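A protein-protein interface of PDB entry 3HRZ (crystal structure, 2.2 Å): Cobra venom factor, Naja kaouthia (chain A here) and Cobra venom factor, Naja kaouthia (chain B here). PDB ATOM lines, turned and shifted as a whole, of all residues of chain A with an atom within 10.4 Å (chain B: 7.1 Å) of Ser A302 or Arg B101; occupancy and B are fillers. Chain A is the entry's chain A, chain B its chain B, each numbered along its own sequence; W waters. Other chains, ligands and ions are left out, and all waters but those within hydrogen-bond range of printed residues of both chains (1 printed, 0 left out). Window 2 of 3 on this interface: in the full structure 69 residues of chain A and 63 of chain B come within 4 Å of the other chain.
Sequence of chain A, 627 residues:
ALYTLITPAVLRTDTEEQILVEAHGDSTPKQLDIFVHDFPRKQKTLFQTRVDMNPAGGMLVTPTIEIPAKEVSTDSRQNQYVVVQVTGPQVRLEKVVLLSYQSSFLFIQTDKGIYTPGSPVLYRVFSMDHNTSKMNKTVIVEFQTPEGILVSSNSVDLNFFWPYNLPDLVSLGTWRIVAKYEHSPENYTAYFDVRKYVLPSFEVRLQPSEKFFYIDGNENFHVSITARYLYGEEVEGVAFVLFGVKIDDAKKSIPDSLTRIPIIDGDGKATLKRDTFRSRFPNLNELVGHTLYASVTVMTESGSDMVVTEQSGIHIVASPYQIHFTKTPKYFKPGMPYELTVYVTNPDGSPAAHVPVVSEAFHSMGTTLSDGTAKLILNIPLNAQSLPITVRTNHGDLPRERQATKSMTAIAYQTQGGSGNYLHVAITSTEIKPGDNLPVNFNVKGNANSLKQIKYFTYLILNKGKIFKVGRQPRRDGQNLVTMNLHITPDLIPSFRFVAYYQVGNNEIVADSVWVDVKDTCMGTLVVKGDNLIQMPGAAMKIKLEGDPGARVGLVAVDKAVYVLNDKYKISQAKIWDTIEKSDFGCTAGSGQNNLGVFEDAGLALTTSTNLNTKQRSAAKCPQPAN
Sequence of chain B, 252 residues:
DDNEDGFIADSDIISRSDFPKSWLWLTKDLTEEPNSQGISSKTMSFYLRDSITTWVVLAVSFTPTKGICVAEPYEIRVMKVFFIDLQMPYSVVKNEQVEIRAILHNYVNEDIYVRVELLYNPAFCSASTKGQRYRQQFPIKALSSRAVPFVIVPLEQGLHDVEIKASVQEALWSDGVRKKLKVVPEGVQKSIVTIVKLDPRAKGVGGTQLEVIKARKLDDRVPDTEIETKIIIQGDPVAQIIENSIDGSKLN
Water W1 lies within hydrogen-bond range of OD1 of Asp A305 and NE2 of Gln B87.
Asp B85 touches Ser A201.
Ser A201 touches Gln B87 (CB to OE1, 3.7 Å).
Ser A302 touches Ile B103.
O of Ser A304 touches CB of Gln B87 (3.6 Å).
Ile B103 touches Ser A304 (CG1 to OG, 3.6 Å).
Gln B87 touches Asp A305.
The backbone carbonyl oxygen (O) of Asp A305 lies within hydrogen-bond range of the backbone NH (N) of Thr A300 (2.9 Å).
The side-chain hydroxyl of Ser A201 sits at hydrogen-bond distance from the side-chain carboxylate of Asp A305, 2.6 Å away.
The side-chain carboxylate (OE2) of Glu B99 lies within salt-bridge range of the guanidinium group (NH2) of Arg B101.
N of Asp B85 lies within hydrogen-bond range of O of Ile B103, at 2.8 Å.
The side-chain hydroxyl (OG) of Ser A304 lies within hydrogen-bond range of the side-chain hydroxyl (OG1) of Thr A300, at 3.2 Å.
The side-chain hydroxyl (OG) of Ser A302 lies within hydrogen-bond range of the side-chain hydroxyl (OG) of Ser A304 (3.0 Å).
Glu A236 touches none of the printed residues of chain B.
Of the printed residues of chain B, Ser A304 touches Gln B87 (3.6 Å) and Ile B103 (3.6 Å).
Of the printed residues of chain B, Asp A305 touches Gln B87.
Of the printed residues of chain A, Asp B85 touches Ser A201.
No residue of chain A comes within 4 Å of Ile B100.
Of chain A, only Ser A302 (2.8 Å) comes within 4 Å of Arg B101.
No residue of chain A comes within 4 Å of Ala B102.
Of the printed residues of chain A, Ile B103 touches Ser A302 (3.4 Å) and Ser A304 (3.6 Å).
No residue of chain A comes within 4 Å of Ala B147.
The nearest printed residue of chain B that does not touch Ser A201 is Leu B86 (7.0 Å).
O of Ser A302 sits at hydrogen-bond distance from NH1 of Arg B101 (2.8 Å).
Hydrophobic or aromatic side chains of chain B within 4 Å of the printed part of chain A: Ile B103.
Among the printed residues, no Asp or Glu carboxylate lies within 4 Å of a Lys or Arg side-chain nitrogen of the other chain.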
ATOM      1  N   SER A 201      -8.235  -6.484   7.315  1.00  0.00           N
ATOM      2  CA  SER A 201      -8.050  -7.311   8.500  1.00  0.00           C
ATOM      3  C   SER A 201      -7.302  -6.550   9.608  1.00  0.00           C
ATOM      4  O   SER A 201      -7.160  -7.064  10.733  1.00  0.00           O
ATOM      5  CB  SER A 201      -7.253  -8.560   8.132  1.00  0.00           C
ATOM      6  OG  SER A 201      -6.057  -8.201   7.454  1.00  0.00           O
ATOM      7  N   PHE A 202      -6.832  -5.341   9.308  1.00  0.00           N
ATOM      8  CA  PHE A 202      -6.093  -4.595  10.324  1.00  0.00           C
ATOM      9  C   PHE A 202      -6.320  -3.097  10.248  1.00  0.00           C
ATOM     10  O   PHE A 202      -6.790  -2.569   9.246  1.00  0.00           O
ATOM     11  CB  PHE A 202      -4.592  -4.900  10.269  1.00  0.00           C
ATOM     12  CG  PHE A 202      -3.910  -4.380   9.042  1.00  0.00           C
ATOM     13  CD1 PHE A 202      -3.186  -3.193   9.082  1.00  0.00           C
ATOM     14  CD2 PHE A 202      -3.997  -5.070   7.839  1.00  0.00           C
ATOM     15  CE1 PHE A 202      -2.534  -2.710   7.939  1.00  0.00           C
ATOM     16  CE2 PHE A 202      -3.365  -4.593   6.697  1.00  0.00           C
ATOM     17  CZ  PHE A 202      -2.625  -3.406   6.749  1.00  0.00           C
ATOM     18  N   TYR A 229      -3.823  -5.846  13.891  1.00  0.00           N
ATOM     19  CA  TYR A 229      -4.954  -6.588  13.401  1.00  0.00           C
ATOM     20  C   TYR A 229      -6.112  -6.229  14.305  1.00  0.00           C
ATOM     21  O   TYR A 229      -5.904  -5.920  15.468  1.00  0.00           O
ATOM     22  CB  TYR A 229      -4.687  -8.079  13.489  1.00  0.00           C
ATOM     23  CG  TYR A 229      -3.680  -8.550  12.481  1.00  0.00           C
ATOM     24  CD1 TYR A 229      -4.018  -8.649  11.133  1.00  0.00           C
ATOM     25  CD2 TYR A 229      -2.385  -8.886  12.872  1.00  0.00           C
ATOM     26  CE1 TYR A 229      -3.097  -9.078  10.192  1.00  0.00           C
ATOM     27  CE2 TYR A 229      -1.449  -9.333  11.939  1.00  0.00           C
ATOM     28  CZ  TYR A 229      -1.816  -9.426  10.602  1.00  0.00           C
ATOM     29  OH  TYR A 229      -0.900  -9.853   9.679  1.00  0.00           O
ATOM     30  N   VAL A 235       1.011  -6.183  13.466  1.00  0.00           N
ATOM     31  CA  VAL A 235       1.215  -6.420  12.052  1.00  0.00           C
ATOM     32  C   VAL A 235       2.689  -6.272  11.691  1.00  0.00           C
ATOM     33  O   VAL A 235       3.378  -5.333  12.146  1.00  0.00           O
ATOM     34  CB  VAL A 235       0.390  -5.440  11.191  1.00  0.00           C
ATOM     35  CG1 VAL A 235       0.693  -5.651   9.704  1.00  0.00           C
ATOM     36  CG2 VAL A 235      -1.105  -5.618  11.444  1.00  0.00           C
ATOM     37  N   GLU A 236       3.185  -7.215  10.894  1.00  0.00           N
ATOM     38  CA  GLU A 236       4.496  -7.081  10.252  1.00  0.00           C
ATOM     39  C   GLU A 236       4.310  -6.825   8.756  1.00  0.00           C
ATOM     40  O   GLU A 236       3.486  -7.479   8.083  1.00  0.00           O
ATOM     41  CB  GLU A 236       5.374  -8.320  10.487  1.00  0.00           C
ATOM     42  CG  GLU A 236       6.734  -8.257   9.777  1.00  0.00           C
ATOM     43  CD  GLU A 236       7.818  -9.130  10.433  1.00  0.00           C
ATOM     44  OE1 GLU A 236       8.389  -8.708  11.469  1.00  0.00           O
ATOM     45  OE2 GLU A 236       8.118 -10.226   9.900  1.00  0.00           O
ATOM     46  N   GLY A 237       5.054  -5.870   8.232  1.00  0.00           N
ATOM     47  CA  GLY A 237       4.928  -5.534   6.831  1.00  0.00           C
ATOM     48  C   GLY A 237       5.754  -4.327   6.438  1.00  0.00           C
ATOM     49  O   GLY A 237       6.852  -4.122   6.940  1.00  0.00           O
ATOM     50  N   VAL A 238       5.207  -3.528   5.537  1.00  0.00           N
ATOM     51  CA  VAL A 238       5.915  -2.402   4.940  1.00  0.00           C
ATOM     52  C   VAL A 238       4.928  -1.242   4.787  1.00  0.00           C
ATOM     53  O   VAL A 238       3.729  -1.469   4.605  1.00  0.00           O
ATOM     54  CB  VAL A 238       6.514  -2.810   3.561  1.00  0.00           C
ATOM     55  CG1 VAL A 238       7.044  -1.614   2.818  1.00  0.00           C
ATOM     56  CG2 VAL A 238       7.637  -3.858   3.740  1.00  0.00           C
ATOM     57  N   ILE A 263       7.489  -2.183   8.723  1.00  0.00           N
ATOM     58  CA  ILE A 263       6.597  -2.214   9.860  1.00  0.00           C
ATOM     59  C   ILE A 263       6.914  -3.479  10.648  1.00  0.00           C
ATOM     60  O   ILE A 263       6.552  -4.591  10.250  1.00  0.00           O
ATOM     61  CB  ILE A 263       5.120  -2.163   9.430  1.00  0.00           C
ATOM     62  CG1 ILE A 263       4.849  -0.857   8.700  1.00  0.00           C
ATOM     63  CG2 ILE A 263       4.205  -2.227  10.644  1.00  0.00           C
ATOM     64  CD1 ILE A 263       5.045   0.358   9.576  1.00  0.00           C
ATOM     65  N   VAL A 298      -0.088   0.859   4.126  1.00  0.00           N
ATOM     66  CA  VAL A 298       0.593  -0.255   4.778  1.00  0.00           C
ATOM     67  C   VAL A 298       0.198  -1.576   4.111  1.00  0.00           C
ATOM     68  O   VAL A 298      -0.989  -1.817   3.881  1.00  0.00           O
ATOM     69  CB  VAL A 298       0.246  -0.315   6.274  1.00  0.00           C
ATOM     70  CG1 VAL A 298       0.853  -1.566   6.934  1.00  0.00           C
ATOM     71  CG2 VAL A 298       0.727   0.967   6.986  1.00  0.00           C
ATOM     72  N   MET A 299       1.190  -2.416   3.802  1.00  0.00           N
ATOM     73  CA  MET A 299       0.945  -3.776   3.306  1.00  0.00           C
ATOM     74  C   MET A 299       1.445  -4.809   4.303  1.00  0.00           C
ATOM     75  O   MET A 299       2.526  -4.643   4.875  1.00  0.00           O
ATOM     76  CB  MET A 299       1.670  -3.998   1.982  1.00  0.00           C
ATOM     77  CG  MET A 299       1.292  -2.984   0.943  1.00  0.00           C
ATOM     78  SD  MET A 299       2.445  -2.956  -0.412  1.00  0.00           S
ATOM     79  CE  MET A 299       1.849  -1.532  -1.320  1.00  0.00           C
ATOM     80  N   THR A 300       0.693  -5.887   4.503  1.00  0.00           N
ATOM     81  CA  THR A 300       1.197  -6.948   5.370  1.00  0.00           C
ATOM     82  C   THR A 300       2.391  -7.603   4.676  1.00  0.00           C
ATOM     83  O   THR A 300       2.533  -7.485   3.459  1.00  0.00           O
ATOM     84  CB  THR A 300       0.129  -7.989   5.663  1.00  0.00           C
ATOM     85  OG1 THR A 300      -0.294  -8.579   4.433  1.00  0.00           O
ATOM     86  CG2 THR A 300      -1.091  -7.330   6.328  1.00  0.00           C
ATOM     87  N   GLU A 301       3.242  -8.283   5.439  1.00  0.00           N
ATOM     88  CA  GLU A 301       4.464  -8.861   4.888  1.00  0.00           C
ATOM     89  C   GLU A 301       4.193  -9.894   3.785  1.00  0.00           C
ATOM     90  O   GLU A 301       4.971 -10.020   2.841  1.00  0.00           O
ATOM     91  CB  GLU A 301       5.365  -9.457   5.998  1.00  0.00           C
ATOM     92  CG  GLU A 301       4.718 -10.555   6.839  1.00  0.00           C
ATOM     93  CD  GLU A 301       4.818 -11.939   6.199  1.00  0.00           C
ATOM     94  OE1 GLU A 301       5.470 -12.066   5.140  1.00  0.00           O
ATOM     95  OE2 GLU A 301       4.251 -12.903   6.760  1.00  0.00           O
ATOM     96  N   SER A 302       3.091 -10.626   3.906  1.00  0.00           N
ATOM     97  CA  SER A 302       2.743 -11.661   2.921  1.00  0.00           C
ATOM     98  C   SER A 302       2.039 -11.074   1.700  1.00  0.00           C
ATOM     99  O   SER A 302       1.772 -11.792   0.756  1.00  0.00           O
ATOM    100  CB  SER A 302       1.797 -12.667   3.548  1.00  0.00           C
ATOM    101  OG  SER A 302       0.559 -12.009   3.798  1.00  0.00           O
ATOM    102  N   GLY A 303       1.716  -9.777   1.719  1.00  0.00           N
ATOM    103  CA  GLY A 303       1.020  -9.163   0.590  1.00  0.00           C
ATOM    104  C   GLY A 303      -0.466  -9.523   0.496  1.00  0.00           C
ATOM    105  O   GLY A 303      -1.128  -9.259  -0.509  1.00  0.00           O
ATOM    106  N   SER A 304      -1.001 -10.134   1.545  1.00  0.00           N
ATOM    107  CA  SER A 304      -2.400 -10.542   1.555  1.00  0.00           C
ATOM    108  C   SER A 304      -3.363  -9.370   1.791  1.00  0.00           C
ATOM    109  O   SER A 304      -4.556  -9.481   1.527  1.00  0.00           O
ATOM    110  CB  SER A 304      -2.626 -11.594   2.645  1.00  0.00           C
ATOM    111  OG  SER A 304      -2.277 -11.067   3.919  1.00  0.00           O
ATOM    112  N   ASP A 305      -2.857  -8.258   2.316  1.00  0.00           N
ATOM    113  CA  ASP A 305      -3.735  -7.147   2.654  1.00  0.00           C
ATOM    114  C   ASP A 305      -3.021  -5.794   2.702  1.00  0.00           C
ATOM    115  O   ASP A 305      -1.825  -5.708   2.978  1.00  0.00           O
ATOM    116  CB  ASP A 305      -4.427  -7.440   3.980  1.00  0.00           C
ATOM    117  CG  ASP A 305      -5.764  -6.704   4.133  1.00  0.00           C
ATOM    118  OD1 ASP A 305      -6.246  -6.054   3.169  1.00  0.00           O
ATOM    119  OD2 ASP A 305      -6.333  -6.790   5.244  1.00  0.00           O
ATOM    120  N   MET A 306      -3.789  -4.741   2.450  1.00  0.00           N
ATOM    121  CA  MET A 306      -3.282  -3.387   2.366  1.00  0.00           C
ATOM    122  C   MET A 306      -4.297  -2.409   2.981  1.00  0.00           C
ATOM    123  O   MET A 306      -5.512  -2.576   2.825  1.00  0.00           O
ATOM    124  CB  MET A 306      -3.070  -3.039   0.888  1.00  0.00           C
ATOM    125  CG  MET A 306      -2.409  -1.697   0.642  1.00  0.00           C
ATOM    126  SD  MET A 306      -2.079  -1.428  -1.116  1.00  0.00           S
ATOM    127  CE  MET A 306      -3.697  -1.701  -1.813  1.00  0.00           C
ATOM    128  N   ASP B  85      -7.325 -16.663   8.209  1.00  0.00           N
ATOM    129  CA  ASP B  85      -7.708 -15.303   7.856  1.00  0.00           C
ATOM    130  C   ASP B  85      -7.794 -15.268   6.341  1.00  0.00           C
ATOM    131  O   ASP B  85      -6.832 -15.590   5.646  1.00  0.00           O
ATOM    132  CB  ASP B  85      -6.654 -14.314   8.381  1.00  0.00           C
ATOM    133  CG  ASP B  85      -6.841 -12.903   7.843  1.00  0.00           C
ATOM    134  OD1 ASP B  85      -7.991 -12.528   7.513  1.00  0.00           O
ATOM    135  OD2 ASP B  85      -5.830 -12.163   7.761  1.00  0.00           O
ATOM    136  N   LEU B  86      -8.946 -14.903   5.813  1.00  0.00           N
ATOM    137  CA  LEU B  86      -9.125 -15.028   4.381  1.00  0.00           C
ATOM    138  C   LEU B  86      -9.580 -13.712   3.794  1.00  0.00           C
ATOM    139  O   LEU B  86     -10.759 -13.361   3.883  1.00  0.00           O
ATOM    140  CB  LEU B  86     -10.114 -16.160   4.069  1.00  0.00           C
ATOM    141  CG  LEU B  86     -10.619 -16.354   2.638  1.00  0.00           C
ATOM    142  CD1 LEU B  86      -9.476 -16.499   1.655  1.00  0.00           C
ATOM    143  CD2 LEU B  86     -11.548 -17.582   2.568  1.00  0.00           C
ATOM    144  N   GLN B  87      -8.635 -12.963   3.235  1.00  0.00           N
ATOM    145  CA  GLN B  87      -8.972 -11.738   2.516  1.00  0.00           C
ATOM    146  C   GLN B  87      -9.346 -12.041   1.069  1.00  0.00           C
ATOM    147  O   GLN B  87      -8.556 -12.614   0.319  1.00  0.00           O
ATOM    148  CB  GLN B  87      -7.813 -10.743   2.554  1.00  0.00           C
ATOM    149  CG  GLN B  87      -7.606 -10.108   3.916  1.00  0.00           C
ATOM    150  CD  GLN B  87      -8.845  -9.388   4.429  1.00  0.00           C
ATOM    151  OE1 GLN B  87      -9.428  -9.785   5.444  1.00  0.00           O
ATOM    152  NE2 GLN B  87      -9.256  -8.325   3.728  1.00  0.00           N
ATOM    153  N   MET B  88     -10.558 -11.663   0.686  1.00  0.00           N
ATOM    154  CA  MET B  88     -11.047 -11.886  -0.667  1.00  0.00           C
ATOM    155  C   MET B  88     -11.055 -10.556  -1.400  1.00  0.00           C
ATOM    156  O   MET B  88     -11.310  -9.526  -0.794  1.00  0.00           O
ATOM    157  CB  MET B  88     -12.482 -12.436  -0.634  1.00  0.00           C
ATOM    158  CG  MET B  88     -12.669 -13.764   0.103  1.00  0.00           C
ATOM    159  SD  MET B  88     -12.311 -15.235  -0.903  1.00  0.00           S
ATOM    160  CE  MET B  88     -13.399 -16.429  -0.134  1.00  0.00           C
ATOM    161  N   PRO B  89     -10.799 -10.581  -2.712  1.00  0.00           N
ATOM    162  CA  PRO B  89     -10.949  -9.417  -3.592  1.00  0.00           C
ATOM    163  C   PRO B  89     -12.431  -9.056  -3.680  1.00  0.00           C
ATOM    164  O   PRO B  89     -13.283  -9.904  -3.403  1.00  0.00           O
ATOM    165  CB  PRO B  89     -10.477  -9.961  -4.946  1.00  0.00           C
ATOM    166  CG  PRO B  89     -10.816 -11.421  -4.857  1.00  0.00           C
ATOM    167  CD  PRO B  89     -10.428 -11.790  -3.472  1.00  0.00           C
ATOM    168  N   GLU B  99      -5.462 -16.403  -7.839  1.00  0.00           N
ATOM    169  CA  GLU B  99      -4.954 -16.957  -6.598  1.00  0.00           C
ATOM    170  C   GLU B  99      -5.602 -16.265  -5.402  1.00  0.00           C
ATOM    171  O   GLU B  99      -5.655 -15.035  -5.340  1.00  0.00           O
ATOM    172  CB  GLU B  99      -3.453 -16.752  -6.497  1.00  0.00           C
ATOM    173  CG  GLU B  99      -2.947 -17.070  -5.117  1.00  0.00           C
ATOM    174  CD  GLU B  99      -1.521 -16.643  -4.922  1.00  0.00           C
ATOM    175  OE1 GLU B  99      -0.728 -16.830  -5.869  1.00  0.00           O
ATOM    176  OE2 GLU B  99      -1.193 -16.123  -3.828  1.00  0.00           O
ATOM    177  N   ILE B 100      -6.078 -17.070  -4.460  1.00  0.00           N
ATOM    178  CA  ILE B 100      -6.633 -16.594  -3.210  1.00  0.00           C
ATOM    179  C   ILE B 100      -5.582 -16.882  -2.146  1.00  0.00           C
ATOM    180  O   ILE B 100      -5.087 -18.005  -2.049  1.00  0.00           O
ATOM    181  CB  ILE B 100      -7.927 -17.355  -2.846  1.00  0.00           C
ATOM    182  CG1 ILE B 100      -8.980 -17.207  -3.944  1.00  0.00           C
ATOM    183  CG2 ILE B 100      -8.488 -16.833  -1.554  1.00  0.00           C
ATOM    184  CD1 ILE B 100      -9.413 -15.768  -4.181  1.00  0.00           C
ATOM    185  N   ARG B 101      -5.234 -15.880  -1.345  1.00  0.00           N
ATOM    186  CA  ARG B 101      -4.130 -16.046  -0.403  1.00  0.00           C
ATOM    187  C   ARG B 101      -4.592 -16.030   1.042  1.00  0.00           C
ATOM    188  O   ARG B 101      -4.647 -14.981   1.675  1.00  0.00           O
ATOM    189  CB  ARG B 101      -3.047 -14.989  -0.644  1.00  0.00           C
ATOM    190  CG  ARG B 101      -1.762 -15.202   0.163  1.00  0.00           C
ATOM    191  CD  ARG B 101      -0.690 -14.207  -0.268  1.00  0.00           C
ATOM    192  NE  ARG B 101      -0.371 -14.414  -1.676  1.00  0.00           N
ATOM    193  CZ  ARG B 101       0.448 -13.652  -2.388  1.00  0.00           C
ATOM    194  NH1 ARG B 101       1.050 -12.604  -1.830  1.00  0.00           N
ATOM    195  NH2 ARG B 101       0.648 -13.932  -3.672  1.00  0.00           N
ATOM    196  N   ALA B 102      -4.932 -17.206   1.559  1.00  0.00           N
ATOM    197  CA  ALA B 102      -5.288 -17.335   2.959  1.00  0.00           C
ATOM    198  C   ALA B 102      -4.040 -17.213   3.845  1.00  0.00           C
ATOM    199  O   ALA B 102      -2.925 -17.543   3.426  1.00  0.00           O
ATOM    200  CB  ALA B 102      -5.996 -18.655   3.206  1.00  0.00           C
ATOM    201  N   ILE B 103      -4.234 -16.720   5.063  1.00  0.00           N
ATOM    202  CA  ILE B 103      -3.184 -16.715   6.069  1.00  0.00           C
ATOM    203  C   ILE B 103      -3.611 -17.603   7.237  1.00  0.00           C
ATOM    204  O   ILE B 103      -4.726 -17.480   7.742  1.00  0.00           O
ATOM    205  CB  ILE B 103      -2.894 -15.298   6.608  1.00  0.00           C
ATOM    206  CG1 ILE B 103      -2.498 -14.334   5.480  1.00  0.00           C
ATOM    207  CG2 ILE B 103      -1.807 -15.356   7.659  1.00  0.00           C
ATOM    208  CD1 ILE B 103      -1.262 -14.761   4.689  1.00  0.00           C
ATOM    209  N   ARG B 146       1.441 -18.114   8.339  1.00  0.00           N
ATOM    210  CA  ARG B 146       1.905 -18.763   7.134  1.00  0.00           C
ATOM    211  C   ARG B 146       0.891 -18.503   6.043  1.00  0.00           C
ATOM    212  O   ARG B 146      -0.294 -18.748   6.233  1.00  0.00           O
ATOM    213  CB  ARG B 146       2.064 -20.267   7.373  1.00  0.00           C
ATOM    214  CG  ARG B 146       2.639 -21.049   6.192  1.00  0.00           C
ATOM    215  CD  ARG B 146       4.113 -20.725   5.953  1.00  0.00           C
ATOM    216  NE  ARG B 146       4.965 -21.008   7.109  1.00  0.00           N
ATOM    217  CZ  ARG B 146       6.016 -21.826   7.088  1.00  0.00           C
ATOM    218  NH1 ARG B 146       6.354 -22.453   5.968  1.00  0.00           N
ATOM    219  NH2 ARG B 146       6.736 -22.016   8.189  1.00  0.00           N
ATOM    220  N   ALA B 147       1.352 -17.980   4.912  1.00  0.00           N
ATOM    221  CA  ALA B 147       0.502 -17.843   3.734  1.00  0.00           C
ATOM    222  C   ALA B 147       0.181 -19.222   3.154  1.00  0.00           C
ATOM    223  O   ALA B 147       1.057 -20.082   3.074  1.00  0.00           O
ATOM    224  CB  ALA B 147       1.175 -16.970   2.688  1.00  0.00           C
ATOM    225  N   VAL B 148      -1.079 -19.417   2.771  1.00  0.00           N
ATOM    226  CA  VAL B 148      -1.544 -20.645   2.128  1.00  0.00           C
ATOM    227  C   VAL B 148      -2.375 -20.268   0.917  1.00  0.00           C
ATOM    228  O   VAL B 148      -3.570 -19.991   1.033  1.00  0.00           O
ATOM    229  CB  VAL B 148      -2.414 -21.476   3.061  1.00  0.00           C
ATOM    230  CG1 VAL B 148      -2.784 -22.818   2.400  1.00  0.00           C
ATOM    231  CG2 VAL B 148      -1.708 -21.686   4.411  1.00  0.00           C
ATOM    232  N   PRO B 149      -1.728 -20.214  -0.250  1.00  0.00           N
ATOM    233  CA  PRO B 149      -2.314 -19.885  -1.553  1.00  0.00           C
ATOM    234  C   PRO B 149      -3.277 -20.976  -2.038  1.00  0.00           C
ATOM    235  O   PRO B 149      -3.011 -22.155  -1.853  1.00  0.00           O
ATOM    236  CB  PRO B 149      -1.096 -19.857  -2.489  1.00  0.00           C
ATOM    237  CG  PRO B 149       0.088 -19.723  -1.595  1.00  0.00           C
ATOM    238  CD  PRO B 149      -0.274 -20.421  -0.327  1.00  0.00           C
ATOM    239  N   PHE B 150      -4.388 -20.571  -2.638  1.00  0.00           N
ATOM    240  CA  PHE B 150      -5.258 -21.507  -3.330  1.00  0.00           C
ATOM    241  C   PHE B 150      -5.550 -20.955  -4.695  1.00  0.00           C
ATOM    242  O   PHE B 150      -5.896 -19.782  -4.830  1.00  0.00           O
ATOM    243  CB  PHE B 150      -6.535 -21.745  -2.535  1.00  0.00           C
ATOM    244  CG  PHE B 150      -6.299 -22.508  -1.278  1.00  0.00           C
ATOM    245  CD1 PHE B 150      -6.030 -23.869  -1.328  1.00  0.00           C
ATOM    246  CD2 PHE B 150      -6.293 -21.869  -0.059  1.00  0.00           C
ATOM    247  CE1 PHE B 150      -5.787 -24.587  -0.167  1.00  0.00           C
ATOM    248  CE2 PHE B 150      -6.057 -22.576   1.104  1.00  0.00           C
ATOM    249  CZ  PHE B 150      -5.804 -23.936   1.051  1.00  0.00           C
ATOM    250  N   ILE B 164     -12.344 -23.148   3.448  1.00  0.00           N
ATOM    251  CA  ILE B 164     -11.070 -23.723   3.869  1.00  0.00           C
ATOM    252  C   ILE B 164     -11.158 -24.166   5.323  1.00  0.00           C
ATOM    253  O   ILE B 164     -11.759 -23.488   6.144  1.00  0.00           O
ATOM    254  CB  ILE B 164      -9.957 -22.691   3.712  1.00  0.00           C
ATOM    255  CG1 ILE B 164      -9.945 -22.178   2.274  1.00  0.00           C
ATOM    256  CG2 ILE B 164      -8.606 -23.272   4.100  1.00  0.00           C
ATOM    257  CD1 ILE B 164      -9.145 -20.896   2.113  1.00  0.00           C
HETATM  258  O   HOH W   1      -8.913  -5.787   2.461  1.00  0.00           O
